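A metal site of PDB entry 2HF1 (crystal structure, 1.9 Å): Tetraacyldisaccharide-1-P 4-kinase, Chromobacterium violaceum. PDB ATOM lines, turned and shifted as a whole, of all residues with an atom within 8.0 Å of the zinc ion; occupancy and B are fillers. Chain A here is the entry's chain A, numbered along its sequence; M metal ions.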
ATOM      1  N   VAL A  10      -7.607  -5.716   8.681  1.00  0.00           N
ATOM      2  CA  VAL A  10      -6.658  -6.474   7.901  1.00  0.00           C
ATOM      3  C   VAL A  10      -7.439  -7.650   7.332  1.00  0.00           C
ATOM      4  O   VAL A  10      -8.484  -8.043   7.878  1.00  0.00           O
ATOM      5  CB  VAL A  10      -5.459  -7.015   8.742  1.00  0.00           C
ATOM      6  CG1 VAL A  10      -4.532  -5.867   9.097  1.00  0.00           C
ATOM      7  CG2 VAL A  10      -5.954  -7.710   9.996  1.00  0.00           C
ATOM      8  N   CYS A  11      -6.954  -8.210   6.235  1.00  0.00           N
ATOM      9  CA  CYS A  11      -7.624  -9.343   5.618  1.00  0.00           C
ATOM     10  C   CYS A  11      -7.669 -10.496   6.602  1.00  0.00           C
ATOM     11  O   CYS A  11      -6.650 -10.869   7.180  1.00  0.00           O
ATOM     12  CB  CYS A  11      -6.887  -9.777   4.351  1.00  0.00           C
ATOM     13  SG  CYS A  11      -7.586 -11.273   3.664  1.00  0.00           S
ATOM     14  N   PRO A  12      -8.854 -11.099   6.806  1.00  0.00           N
ATOM     15  CA  PRO A  12      -8.971 -12.219   7.744  1.00  0.00           C
ATOM     16  C   PRO A  12      -8.119 -13.435   7.383  1.00  0.00           C
ATOM     17  O   PRO A  12      -7.955 -14.346   8.183  1.00  0.00           O
ATOM     18  CB  PRO A  12     -10.468 -12.534   7.711  1.00  0.00           C
ATOM     19  CG  PRO A  12     -10.853 -12.170   6.337  1.00  0.00           C
ATOM     20  CD  PRO A  12     -10.134 -10.854   6.124  1.00  0.00           C
ATOM     21  N   LEU A  13      -7.564 -13.439   6.166  1.00  0.00           N
ATOM     22  CA  LEU A  13      -6.725 -14.548   5.719  1.00  0.00           C
ATOM     23  C   LEU A  13      -5.221 -14.307   5.823  1.00  0.00           C
ATOM     24  O   LEU A  13      -4.532 -14.940   6.623  1.00  0.00           O
ATOM     25  CB  LEU A  13      -7.068 -14.925   4.281  1.00  0.00           C
ATOM     26  CG  LEU A  13      -8.359 -15.719   4.057  1.00  0.00           C
ATOM     27  CD1 LEU A  13      -8.577 -15.955   2.575  1.00  0.00           C
ATOM     28  CD2 LEU A  13      -8.269 -17.040   4.799  1.00  0.00           C
ATOM     29  N   CYS A  14      -4.708 -13.397   5.006  1.00  0.00           N
ATOM     30  CA  CYS A  14      -3.281 -13.091   4.968  1.00  0.00           C
ATOM     31  C   CYS A  14      -2.844 -12.033   5.975  1.00  0.00           C
ATOM     32  O   CYS A  14      -1.650 -11.786   6.148  1.00  0.00           O
ATOM     33  CB  CYS A  14      -2.885 -12.630   3.571  1.00  0.00           C
ATOM     34  SG  CYS A  14      -3.556 -11.005   3.117  1.00  0.00           S
ATOM     35  N   LYS A  15      -3.812 -11.411   6.647  1.00  0.00           N
ATOM     36  CA  LYS A  15      -3.529 -10.349   7.619  1.00  0.00           C
ATOM     37  C   LYS A  15      -2.906  -9.114   6.976  1.00  0.00           C
ATOM     38  O   LYS A  15      -2.265  -8.313   7.656  1.00  0.00           O
ATOM     39  CB  LYS A  15      -2.614 -10.870   8.734  1.00  0.00           C
ATOM     40  CG  LYS A  15      -3.350 -11.586   9.846  1.00  0.00           C
ATOM     41  CD  LYS A  15      -4.102 -12.794   9.310  1.00  0.00           C
ATOM     42  CE  LYS A  15      -5.021 -13.383  10.377  1.00  0.00           C
ATOM     43  NZ  LYS A  15      -4.303 -13.801  11.622  1.00  0.00           N
ATOM     44  N   GLY A  16      -3.095  -8.962   5.666  1.00  0.00           N
ATOM     45  CA  GLY A  16      -2.554  -7.804   4.979  1.00  0.00           C
ATOM     46  C   GLY A  16      -3.535  -6.641   4.972  1.00  0.00           C
ATOM     47  O   GLY A  16      -4.697  -6.823   5.333  1.00  0.00           O
ATOM     48  N   PRO A  17      -3.101  -5.441   4.574  1.00  0.00           N
ATOM     49  CA  PRO A  17      -3.974  -4.262   4.535  1.00  0.00           C
ATOM     50  C   PRO A  17      -5.055  -4.359   3.467  1.00  0.00           C
ATOM     51  O   PRO A  17      -4.922  -5.110   2.503  1.00  0.00           O
ATOM     52  CB  PRO A  17      -2.991  -3.117   4.258  1.00  0.00           C
ATOM     53  CG  PRO A  17      -1.952  -3.783   3.410  1.00  0.00           C
ATOM     54  CD  PRO A  17      -1.735  -5.094   4.127  1.00  0.00           C
ATOM     55  N   LEU A  18      -6.129  -3.609   3.648  1.00  0.00           N
ATOM     56  CA  LEU A  18      -7.247  -3.616   2.714  1.00  0.00           C
ATOM     57  C   LEU A  18      -7.377  -2.284   1.999  1.00  0.00           C
ATOM     58  O   LEU A  18      -7.031  -1.226   2.546  1.00  0.00           O
ATOM     59  CB  LEU A  18      -8.534  -3.924   3.468  1.00  0.00           C
ATOM     60  CG  LEU A  18      -8.483  -5.257   4.201  1.00  0.00           C
ATOM     61  CD1 LEU A  18      -9.597  -5.356   5.220  1.00  0.00           C
ATOM     62  CD2 LEU A  18      -8.572  -6.377   3.168  1.00  0.00           C
ATOM     63  N   ILE A  28     -11.076  -4.314  -0.031  1.00  0.00           N
ATOM     64  CA  ILE A  28     -10.432  -5.292  -0.892  1.00  0.00           C
ATOM     65  C   ILE A  28      -9.052  -5.774  -0.466  1.00  0.00           C
ATOM     66  O   ILE A  28      -8.200  -4.985  -0.047  1.00  0.00           O
ATOM     67  CB  ILE A  28     -10.311  -4.734  -2.333  1.00  0.00           C
ATOM     68  CG1 ILE A  28     -11.690  -4.322  -2.848  1.00  0.00           C
ATOM     69  CG2 ILE A  28      -9.690  -5.786  -3.288  1.00  0.00           C
ATOM     70  CD1 ILE A  28     -11.669  -3.648  -4.223  1.00  0.00           C
ATOM     71  N   CYS A  29      -8.826  -7.079  -0.568  1.00  0.00           N
ATOM     72  CA  CYS A  29      -7.512  -7.611  -0.274  1.00  0.00           C
ATOM     73  C   CYS A  29      -6.922  -7.919  -1.641  1.00  0.00           C
ATOM     74  O   CYS A  29      -7.359  -8.850  -2.323  1.00  0.00           O
ATOM     75  CB  CYS A  29      -7.552  -8.900   0.538  1.00  0.00           C
ATOM     76  SG  CYS A  29      -5.903  -9.669   0.578  1.00  0.00           S
ATOM     77  N   LYS A  30      -5.940  -7.125  -2.047  1.00  0.00           N
ATOM     78  CA  LYS A  30      -5.293  -7.287  -3.341  1.00  0.00           C
ATOM     79  C   LYS A  30      -4.659  -8.668  -3.486  1.00  0.00           C
ATOM     80  O   LYS A  30      -4.942  -9.385  -4.440  1.00  0.00           O
ATOM     81  CB  LYS A  30      -4.245  -6.188  -3.517  1.00  0.00           C
ATOM     82  CG  LYS A  30      -3.441  -6.232  -4.804  1.00  0.00           C
ATOM     83  CD  LYS A  30      -4.296  -5.960  -6.023  1.00  0.00           C
ATOM     84  CE  LYS A  30      -3.451  -5.874  -7.296  1.00  0.00           C
ATOM     85  NZ  LYS A  30      -2.468  -4.760  -7.235  1.00  0.00           N
ATOM     86  N   GLY A  31      -3.815  -9.044  -2.521  1.00  0.00           N
ATOM     87  CA  GLY A  31      -3.132 -10.319  -2.560  1.00  0.00           C
ATOM     88  C   GLY A  31      -3.993 -11.573  -2.646  1.00  0.00           C
ATOM     89  O   GLY A  31      -3.554 -12.592  -3.163  1.00  0.00           O
ATOM     90  N   ASP A  32      -5.224 -11.500  -2.137  1.00  0.00           N
ATOM     91  CA  ASP A  32      -6.124 -12.647  -2.165  1.00  0.00           C
ATOM     92  C   ASP A  32      -7.262 -12.469  -3.166  1.00  0.00           C
ATOM     93  O   ASP A  32      -8.039 -13.394  -3.395  1.00  0.00           O
ATOM     94  CB  ASP A  32      -6.694 -12.895  -0.769  1.00  0.00           C
ATOM     95  CG  ASP A  32      -5.738 -13.683   0.119  1.00  0.00           C
ATOM     96  OD1 ASP A  32      -5.757 -13.465   1.343  1.00  0.00           O
ATOM     97  OD2 ASP A  32      -4.983 -14.532  -0.409  1.00  0.00           O
ATOM     98  N   ARG A  33      -7.346 -11.292  -3.766  1.00  0.00           N
ATOM     99  CA  ARG A  33      -8.382 -10.992  -4.739  1.00  0.00           C
ATOM    100  C   ARG A  33      -9.764 -11.274  -4.161  1.00  0.00           C
ATOM    101  O   ARG A  33     -10.586 -11.964  -4.764  1.00  0.00           O
ATOM    102  CB  ARG A  33      -8.163 -11.831  -5.999  1.00  0.00           C
ATOM    103  N   LEU A  34     -10.005 -10.713  -2.971  1.00  0.00           N
ATOM    104  CA  LEU A  34     -11.262 -10.870  -2.279  1.00  0.00           C
ATOM    105  C   LEU A  34     -11.782  -9.494  -1.848  1.00  0.00           C
ATOM    106  O   LEU A  34     -10.989  -8.602  -1.537  1.00  0.00           O
ATOM    107  CB  LEU A  34     -11.085 -11.738  -1.034  1.00  0.00           C
ATOM    108  CG  LEU A  34     -10.682 -13.207  -1.195  1.00  0.00           C
ATOM    109  CD1 LEU A  34     -10.488 -13.827   0.171  1.00  0.00           C
ATOM    110  CD2 LEU A  34     -11.746 -13.968  -1.982  1.00  0.00           C
ATOM    111  N   PHE A  36     -14.396  -7.689   0.866  1.00  0.00           N
ATOM    112  CA  PHE A  36     -15.232  -7.874   2.049  1.00  0.00           C
ATOM    113  C   PHE A  36     -16.258  -6.757   2.076  1.00  0.00           C
ATOM    114  O   PHE A  36     -15.953  -5.614   1.750  1.00  0.00           O
ATOM    115  CB  PHE A  36     -14.364  -7.866   3.316  1.00  0.00           C
ATOM    116  CG  PHE A  36     -13.387  -8.991   3.361  1.00  0.00           C
ATOM    117  CD1 PHE A  36     -12.212  -8.935   2.626  1.00  0.00           C
ATOM    118  CD2 PHE A  36     -13.676 -10.154   4.074  1.00  0.00           C
ATOM    119  CE1 PHE A  36     -11.343 -10.012   2.580  1.00  0.00           C
ATOM    120  CE2 PHE A  36     -12.816 -11.246   4.037  1.00  0.00           C
ATOM    121  CZ  PHE A  36     -11.642 -11.171   3.292  1.00  0.00           C
HETATM  122 ZN    ZN M   1      -5.726 -11.280   2.150  1.00  0.00          ZN
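The zinc ion is bound by the side-chain sulfur of Cys 29 (2.3 Å), the side-chain carboxylate of Asp 32 (2.3 Å), the side-chain sulfur of Cys 14 (2.4 Å) and the side-chain sulfur of Cys 11 (2.4 Å).
The backbone NH (N) of Cys 29 sits at hydrogen-bond distance from the backbone carbonyl oxygen (O) of Leu 34.
The side-chain sulfur of Cys 14 lies close to the backbone NH of Gly 16 (3.3 Å).
The backbone NH of Leu 13 sits close to the side-chain sulfur of Cys 11, at 3.3 Å.
The backbone carbonyl oxygen (O) of Gly 16 lies within hydrogen-bond range of the backbone NH (N) of Cys 11 (2.8 Å).
The side-chain sulfur (SG) of Cys 29 lies close to the backbone NH (N) of Gly 31 (3.8 Å).
Of the 17 residues printed, 4 come within 4 Å of the zinc ion.
The nearest printed residue that does not touch the zinc ion is Leu 13 (4.4 Å).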
